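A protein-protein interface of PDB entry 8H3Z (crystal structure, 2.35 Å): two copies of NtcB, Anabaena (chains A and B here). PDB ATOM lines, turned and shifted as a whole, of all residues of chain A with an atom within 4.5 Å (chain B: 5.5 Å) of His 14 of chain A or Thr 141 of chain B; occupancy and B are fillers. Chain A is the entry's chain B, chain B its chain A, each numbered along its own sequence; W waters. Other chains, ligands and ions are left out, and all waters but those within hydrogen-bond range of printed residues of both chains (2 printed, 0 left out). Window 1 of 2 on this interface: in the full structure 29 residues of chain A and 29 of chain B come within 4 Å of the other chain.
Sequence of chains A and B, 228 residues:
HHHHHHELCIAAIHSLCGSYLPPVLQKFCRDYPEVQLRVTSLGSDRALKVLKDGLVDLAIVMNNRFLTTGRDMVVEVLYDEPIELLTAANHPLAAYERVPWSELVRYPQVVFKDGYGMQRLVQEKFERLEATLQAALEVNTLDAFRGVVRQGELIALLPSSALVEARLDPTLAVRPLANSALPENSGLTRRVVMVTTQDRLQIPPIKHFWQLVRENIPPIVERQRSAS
NE2 of His 14 of chain B is in hydrogen-bond range of OH of Tyr 116 of chain B (3.1 Å). NE2 of His 14 of chain B sits at hydrogen-bond distance from O of Asn 140 of chain B (3.3 Å). N of Asp 143 of chain B lies close to OG1 of Thr 141 of chain B. N of Ala 144 of chain B is in hydrogen-bond range of OG1 of Thr 141 of chain B (3.2 Å). The side-chain hydroxyl (OH) of Tyr 116 of chain A sits at hydrogen-bond distance from a ring nitrogen (NE2) of His 14 of chain A, at 3.1 Å. NE2 of His 14 of chain A sits at hydrogen-bond distance from O of Asn 140 of chain A, 3.1 Å away.
His 14 of chain A touches Thr 141 of chain B, and with the chains exchanged Thr 141 of chain A touches His 14 of chain B. Positions printed for both chains: 14, 116, 140, 141 and 142. Of the 5 pairs that touch across the chains among the printed residues, 2 have their exchanged pair printed and touching as well.
Ile 13 of chain A touches none of the printed residues of chain B. Of chain B, only Thr 141 comes within 4 Å of His 14 of chain A. Printed residues of chain A within 4 Å of His 14 of chain B: Thr 141. Leu 142 of chain B touches none of the printed residues of chain A. Of the printed residues of chain A, Asp 143 of chain B touches Leu 142 (3.2 Å). The nearest residue of chain B that does not touch His 14 of chain A is Asn 140 of chain B (5.3 Å).
Among the printed residues, merely in contact across the chains: Leu 142 of chain A with Asp 143 of chain B (3.2 Å), Cys 17 of chain A with Ala 144 of chain B (3.6 Å), Thr 141 of chain A with His 14 of chain B (3.8 Å) and His 14 of chain A with Thr 141 of chain B (3.9 Å).
Printed residues of chain A that touch a printed residue of chain B: His 14, Cys 17, Ser 41, Thr 141 and Leu 142. Of the 10 printed residues of chain B, 5 touch a printed residue of chain A. Hydrophobic or aromatic side chains of chain B that line the printed part of chain A: His 14 and Ala 144. Among the printed residues, 5 pairs touch across the chains.
Water W2 bridges OG of Ser 41 of chain A and OD1 of Asn 140 of chain B. Water W1 lies within hydrogen-bond range of the backbone NH of Leu 142 of chain A (2.8 Å), the side-chain carboxylate of Asp 143 of chain B (2.9 Å) and a ring nitrogen (ND1) of His 14 of chain A (3.2 Å).
The backbone NH (N) of Ser 41 of chain A lies within hydrogen-bond range of the side-chain amide oxygen (OD1) of Asn 140 of chain B, at 2.7 Å.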
ATOM      1  N   ALA A  12      -7.920   4.539   7.382  1.00  0.00           N
ATOM      2  CA  ALA A  12      -9.058   5.074   8.147  1.00  0.00           C
ATOM      3  C   ALA A  12      -8.802   5.121   9.648  1.00  0.00           C
ATOM      4  O   ALA A  12      -8.057   4.275  10.149  1.00  0.00           O
ATOM      5  CB  ALA A  12     -10.302   4.287   7.842  1.00  0.00           C
ATOM      6  N   ILE A  13      -9.413   6.099  10.309  1.00  0.00           N
ATOM      7  CA  ILE A  13      -9.366   6.234  11.785  1.00  0.00           C
ATOM      8  C   ILE A  13      -9.871   4.933  12.407  1.00  0.00           C
ATOM      9  O   ILE A  13     -10.807   4.347  11.854  1.00  0.00           O
ATOM     10  CB  ILE A  13     -10.238   7.446  12.174  1.00  0.00           C
ATOM     11  CG1 ILE A  13      -9.547   8.773  11.857  1.00  0.00           C
ATOM     12  CG2 ILE A  13     -10.668   7.380  13.628  1.00  0.00           C
ATOM     13  CD1 ILE A  13     -10.360   9.980  12.260  1.00  0.00           C
ATOM     14  N   HIS A  14      -9.290   4.532  13.533  1.00  0.00           N
ATOM     15  CA  HIS A  14      -9.620   3.236  14.180  1.00  0.00           C
ATOM     16  C   HIS A  14     -11.122   3.111  14.422  1.00  0.00           C
ATOM     17  O   HIS A  14     -11.656   2.027  14.198  1.00  0.00           O
ATOM     18  CB  HIS A  14      -8.788   3.096  15.463  1.00  0.00           C
ATOM     19  CG  HIS A  14      -7.376   2.667  15.245  1.00  0.00           C
ATOM     20  ND1 HIS A  14      -7.037   1.364  14.958  1.00  0.00           N
ATOM     21  CD2 HIS A  14      -6.218   3.356  15.284  1.00  0.00           C
ATOM     22  CE1 HIS A  14      -5.733   1.270  14.823  1.00  0.00           C
ATOM     23  NE2 HIS A  14      -5.210   2.477  15.012  1.00  0.00           N
ATOM     24  N   SER A  15     -11.762   4.199  14.817  1.00  0.00           N
ATOM     25  CA  SER A  15     -13.207   4.200  15.147  1.00  0.00           C
ATOM     26  C   SER A  15     -14.115   3.793  13.987  1.00  0.00           C
ATOM     27  O   SER A  15     -15.155   3.255  14.271  1.00  0.00           O
ATOM     28  CB  SER A  15     -13.603   5.581  15.633  1.00  0.00           C
ATOM     29  OG  SER A  15     -13.392   6.556  14.632  1.00  0.00           O
ATOM     30  N   LEU A  16     -13.674   3.910  12.741  1.00  0.00           N
ATOM     31  CA  LEU A  16     -14.632   3.787  11.652  1.00  0.00           C
ATOM     32  C   LEU A  16     -15.007   2.341  11.328  1.00  0.00           C
ATOM     33  O   LEU A  16     -16.153   2.110  10.964  1.00  0.00           O
ATOM     34  CB  LEU A  16     -14.134   4.560  10.437  1.00  0.00           C
ATOM     35  CG  LEU A  16     -14.479   6.053  10.501  1.00  0.00           C
ATOM     36  CD1 LEU A  16     -13.589   6.867   9.602  1.00  0.00           C
ATOM     37  CD2 LEU A  16     -15.919   6.303  10.119  1.00  0.00           C
ATOM     38  N   CYS A  17     -14.138   1.366  11.571  1.00  0.00           N
ATOM     39  CA  CYS A  17     -14.452  -0.040  11.173  1.00  0.00           C
ATOM     40  C   CYS A  17     -15.355  -0.752  12.201  1.00  0.00           C
ATOM     41  O   CYS A  17     -15.740  -1.887  11.927  1.00  0.00           O
ATOM     42  CB  CYS A  17     -13.176  -0.844  10.935  1.00  0.00           C
ATOM     43  SG  CYS A  17     -12.348  -0.531   9.358  1.00  0.00           S
ATOM     44  N   SER A  41      -6.406   0.581   9.386  1.00  0.00           N
ATOM     45  CA  SER A  41      -6.669   1.485  10.489  1.00  0.00           C
ATOM     46  C   SER A  41      -5.354   2.114  10.967  1.00  0.00           C
ATOM     47  O   SER A  41      -4.437   1.411  11.419  1.00  0.00           O
ATOM     48  CB  SER A  41      -7.423   0.763  11.609  1.00  0.00           C
ATOM     49  OG  SER A  41      -8.599   0.122  11.107  1.00  0.00           O
ATOM     50  N   LEU A  42      -5.328   3.455  10.934  1.00  0.00           N
ATOM     51  CA  LEU A  42      -4.131   4.259  11.138  1.00  0.00           C
ATOM     52  C   LEU A  42      -4.475   5.547  11.896  1.00  0.00           C
ATOM     53  O   LEU A  42      -5.595   6.074  11.802  1.00  0.00           O
ATOM     54  CB  LEU A  42      -3.578   4.654   9.762  1.00  0.00           C
ATOM     55  CG  LEU A  42      -2.935   3.551   8.932  1.00  0.00           C
ATOM     56  CD1 LEU A  42      -2.661   4.051   7.525  1.00  0.00           C
ATOM     57  CD2 LEU A  42      -1.650   3.032   9.589  1.00  0.00           C
ATOM     58  N   TYR A 116      -1.336  10.408  16.172  1.00  0.00           N
ATOM     59  CA  TYR A 116      -2.811  10.322  16.261  1.00  0.00           C
ATOM     60  C   TYR A 116      -3.310  11.724  16.617  1.00  0.00           C
ATOM     61  O   TYR A 116      -2.692  12.368  17.451  1.00  0.00           O
ATOM     62  CB  TYR A 116      -3.230   9.242  17.257  1.00  0.00           C
ATOM     63  CG  TYR A 116      -3.019   7.822  16.797  1.00  0.00           C
ATOM     64  CD1 TYR A 116      -1.760   7.251  16.787  1.00  0.00           C
ATOM     65  CD2 TYR A 116      -4.085   7.045  16.378  1.00  0.00           C
ATOM     66  CE1 TYR A 116      -1.561   5.949  16.366  1.00  0.00           C
ATOM     67  CE2 TYR A 116      -3.904   5.739  15.957  1.00  0.00           C
ATOM     68  CZ  TYR A 116      -2.638   5.190  15.950  1.00  0.00           C
ATOM     69  OH  TYR A 116      -2.454   3.908  15.530  1.00  0.00           O
ATOM     70  N   ASN A 140      -1.942   2.241  20.746  1.00  0.00           N
ATOM     71  CA  ASN A 140      -2.266   2.576  19.368  1.00  0.00           C
ATOM     72  C   ASN A 140      -3.490   1.820  18.828  1.00  0.00           C
ATOM     73  O   ASN A 140      -3.680   1.829  17.610  1.00  0.00           O
ATOM     74  CB  ASN A 140      -1.056   2.328  18.454  1.00  0.00           C
ATOM     75  CG  ASN A 140      -0.774   0.858  18.221  1.00  0.00           C
ATOM     76  OD1 ASN A 140      -1.017   0.036  19.099  1.00  0.00           O
ATOM     77  ND2 ASN A 140      -0.262   0.518  17.048  1.00  0.00           N
ATOM     78  N   THR A 141      -4.335   1.211  19.692  1.00  0.00           N
ATOM     79  CA  THR A 141      -5.569   0.579  19.240  1.00  0.00           C
ATOM     80  C   THR A 141      -6.685   0.775  20.269  1.00  0.00           C
ATOM     81  O   THR A 141      -6.430   0.949  21.457  1.00  0.00           O
ATOM     82  CB  THR A 141      -5.413  -0.926  18.974  1.00  0.00           C
ATOM     83  OG1 THR A 141      -5.240  -1.624  20.208  1.00  0.00           O
ATOM     84  CG2 THR A 141      -4.284  -1.270  18.026  1.00  0.00           C
ATOM     85  N   LEU A 142      -7.939   0.706  19.818  1.00  0.00           N
ATOM     86  CA  LEU A 142      -9.069   0.846  20.730  1.00  0.00           C
ATOM     87  C   LEU A 142      -9.199  -0.363  21.656  1.00  0.00           C
ATOM     88  O   LEU A 142      -9.532  -0.179  22.827  1.00  0.00           O
ATOM     89  CB  LEU A 142     -10.335   1.076  19.912  1.00  0.00           C
ATOM     90  CG  LEU A 142     -10.360   2.406  19.161  1.00  0.00           C
ATOM     91  CD1 LEU A 142     -11.592   2.511  18.271  1.00  0.00           C
ATOM     92  CD2 LEU A 142     -10.290   3.569  20.137  1.00  0.00           C
ATOM     93  N   HIS B  14      -1.703  -8.148  17.866  1.00  0.00           N
ATOM     94  CA  HIS B  14      -2.918  -7.500  18.347  1.00  0.00           C
ATOM     95  C   HIS B  14      -3.616  -8.262  19.484  1.00  0.00           C
ATOM     96  O   HIS B  14      -4.274  -7.632  20.303  1.00  0.00           O
ATOM     97  CB  HIS B  14      -3.876  -7.235  17.183  1.00  0.00           C
ATOM     98  CG  HIS B  14      -3.399  -6.121  16.336  1.00  0.00           C
ATOM     99  ND1 HIS B  14      -3.829  -4.838  16.551  1.00  0.00           N
ATOM    100  CD2 HIS B  14      -2.499  -6.055  15.358  1.00  0.00           C
ATOM    101  CE1 HIS B  14      -3.219  -4.025  15.702  1.00  0.00           C
ATOM    102  NE2 HIS B  14      -2.421  -4.749  14.945  1.00  0.00           N
ATOM    103  N   TYR B 116       1.508  -9.670   8.533  1.00  0.00           N
ATOM    104  CA  TYR B 116       0.974 -10.436   9.651  1.00  0.00           C
ATOM    105  C   TYR B 116       1.223 -11.919   9.387  1.00  0.00           C
ATOM    106  O   TYR B 116       0.906 -12.434   8.309  1.00  0.00           O
ATOM    107  CB  TYR B 116      -0.519 -10.148   9.851  1.00  0.00           C
ATOM    108  CG  TYR B 116      -0.813  -8.782  10.418  1.00  0.00           C
ATOM    109  CD1 TYR B 116      -0.656  -7.645   9.645  1.00  0.00           C
ATOM    110  CD2 TYR B 116      -1.270  -8.632  11.717  1.00  0.00           C
ATOM    111  CE1 TYR B 116      -0.905  -6.383  10.152  1.00  0.00           C
ATOM    112  CE2 TYR B 116      -1.549  -7.380  12.230  1.00  0.00           C
ATOM    113  CZ  TYR B 116      -1.367  -6.255  11.450  1.00  0.00           C
ATOM    114  OH  TYR B 116      -1.580  -5.008  11.963  1.00  0.00           O
ATOM    115  N   VAL B 139      -7.649  -6.270   6.400  1.00  0.00           N
ATOM    116  CA  VAL B 139      -7.882  -5.486   7.599  1.00  0.00           C
ATOM    117  C   VAL B 139      -6.640  -5.640   8.484  1.00  0.00           C
ATOM    118  O   VAL B 139      -5.826  -6.532   8.234  1.00  0.00           O
ATOM    119  CB  VAL B 139      -9.203  -5.995   8.210  1.00  0.00           C
ATOM    120  CG1 VAL B 139      -9.573  -5.392   9.534  1.00  0.00           C
ATOM    121  CG2 VAL B 139     -10.337  -5.925   7.211  1.00  0.00           C
ATOM    122  N   ASN B 140      -6.482  -4.769   9.491  1.00  0.00           N
ATOM    123  CA  ASN B 140      -5.281  -4.795  10.307  1.00  0.00           C
ATOM    124  C   ASN B 140      -5.574  -4.649  11.807  1.00  0.00           C
ATOM    125  O   ASN B 140      -4.661  -4.364  12.576  1.00  0.00           O
ATOM    126  CB  ASN B 140      -4.295  -3.720   9.837  1.00  0.00           C
ATOM    127  CG  ASN B 140      -4.699  -2.330  10.278  1.00  0.00           C
ATOM    128  OD1 ASN B 140      -5.846  -1.920  10.096  1.00  0.00           O
ATOM    129  ND2 ASN B 140      -3.752  -1.600  10.835  1.00  0.00           N
ATOM    130  N   THR B 141      -6.816  -4.858  12.245  1.00  0.00           N
ATOM    131  CA  THR B 141      -7.116  -4.880  13.669  1.00  0.00           C
ATOM    132  C   THR B 141      -8.297  -5.804  13.928  1.00  0.00           C
ATOM    133  O   THR B 141      -9.111  -6.064  13.034  1.00  0.00           O
ATOM    134  CB  THR B 141      -7.438  -3.502  14.276  1.00  0.00           C
ATOM    135  OG1 THR B 141      -8.764  -3.094  13.956  1.00  0.00           O
ATOM    136  CG2 THR B 141      -6.476  -2.413  13.875  1.00  0.00           C
ATOM    137  N   LEU B 142      -8.366  -6.258  15.180  1.00  0.00           N
ATOM    138  CA  LEU B 142      -9.431  -7.133  15.640  1.00  0.00           C
ATOM    139  C   LEU B 142     -10.753  -6.372  15.702  1.00  0.00           C
ATOM    140  O   LEU B 142     -11.797  -6.929  15.412  1.00  0.00           O
ATOM    141  CB  LEU B 142      -9.013  -7.726  16.985  1.00  0.00           C
ATOM    142  CG  LEU B 142      -7.726  -8.568  16.975  1.00  0.00           C
ATOM    143  CD1 LEU B 142      -7.398  -9.121  18.373  1.00  0.00           C
ATOM    144  CD2 LEU B 142      -7.782  -9.729  15.976  1.00  0.00           C
ATOM    145  N   ASP B 143     -10.723  -5.075  16.017  1.00  0.00           N
ATOM    146  CA  ASP B 143     -11.935  -4.267  15.994  1.00  0.00           C
ATOM    147  C   ASP B 143     -12.585  -4.306  14.610  1.00  0.00           C
ATOM    148  O   ASP B 143     -13.797  -4.467  14.506  1.00  0.00           O
ATOM    149  CB  ASP B 143     -11.640  -2.846  16.481  1.00  0.00           C
ATOM    150  CG  ASP B 143     -11.360  -2.798  17.981  1.00  0.00           C
ATOM    151  OD1 ASP B 143     -11.677  -3.819  18.698  1.00  0.00           O
ATOM    152  OD2 ASP B 143     -10.813  -1.755  18.428  1.00  0.00           O
ATOM    153  N   ALA B 144     -11.775  -4.165  13.550  1.00  0.00           N
ATOM    154  CA  ALA B 144     -12.252  -4.186  12.177  1.00  0.00           C
ATOM    155  C   ALA B 144     -12.772  -5.574  11.811  1.00  0.00           C
ATOM    156  O   ALA B 144     -13.753  -5.704  11.086  1.00  0.00           O
ATOM    157  CB  ALA B 144     -11.135  -3.772  11.234  1.00  0.00           C
ATOM    158  N   PHE B 145     -12.076  -6.612  12.270  1.00  0.00           N
ATOM    159  CA  PHE B 145     -12.532  -7.973  12.054  1.00  0.00           C
ATOM    160  C   PHE B 145     -13.945  -8.145  12.618  1.00  0.00           C
ATOM    161  O   PHE B 145     -14.840  -8.636  11.928  1.00  0.00           O
ATOM    162  CB  PHE B 145     -11.569  -8.976  12.694  1.00  0.00           C
ATOM    163  CG  PHE B 145     -10.448  -9.477  11.812  1.00  0.00           C
ATOM    164  CD1 PHE B 145     -10.702 -10.298  10.725  1.00  0.00           C
ATOM    165  CD2 PHE B 145      -9.128  -9.139  12.079  1.00  0.00           C
ATOM    166  CE1 PHE B 145      -9.658 -10.812   9.967  1.00  0.00           C
ATOM    167  CE2 PHE B 145      -8.082  -9.616  11.298  1.00  0.00           C
ATOM    168  CZ  PHE B 145      -8.352 -10.457  10.237  1.00  0.00           C
ATOM    169  N   ARG B 146     -14.148  -7.728  13.870  1.00  0.00           N
ATOM    170  CA  ARG B 146     -15.460  -7.828  14.505  1.00  0.00           C
ATOM    171  C   ARG B 146     -16.499  -6.954  13.802  1.00  0.00           C
ATOM    172  O   ARG B 146     -17.583  -7.452  13.505  1.00  0.00           O
ATOM    173  CB  ARG B 146     -15.353  -7.520  16.002  1.00  0.00           C
ATOM    174  CG  ARG B 146     -14.616  -8.606  16.776  1.00  0.00           C
ATOM    175  CD  ARG B 146     -14.766  -8.494  18.285  1.00  0.00           C
ATOM    176  NE  ARG B 146     -14.288  -7.237  18.828  1.00  0.00           N
ATOM    177  CZ  ARG B 146     -13.014  -6.903  19.050  1.00  0.00           C
ATOM    178  NH1 ARG B 146     -12.009  -7.697  18.746  1.00  0.00           N
ATOM    179  NH2 ARG B 146     -12.741  -5.726  19.550  1.00  0.00           N
HETATM  180  O   HOH W   1      -8.539  -0.256  17.302  1.00  0.00           O
HETATM  181  O   HOH W   2      -8.831  -1.990   9.582  1.00  0.00           O
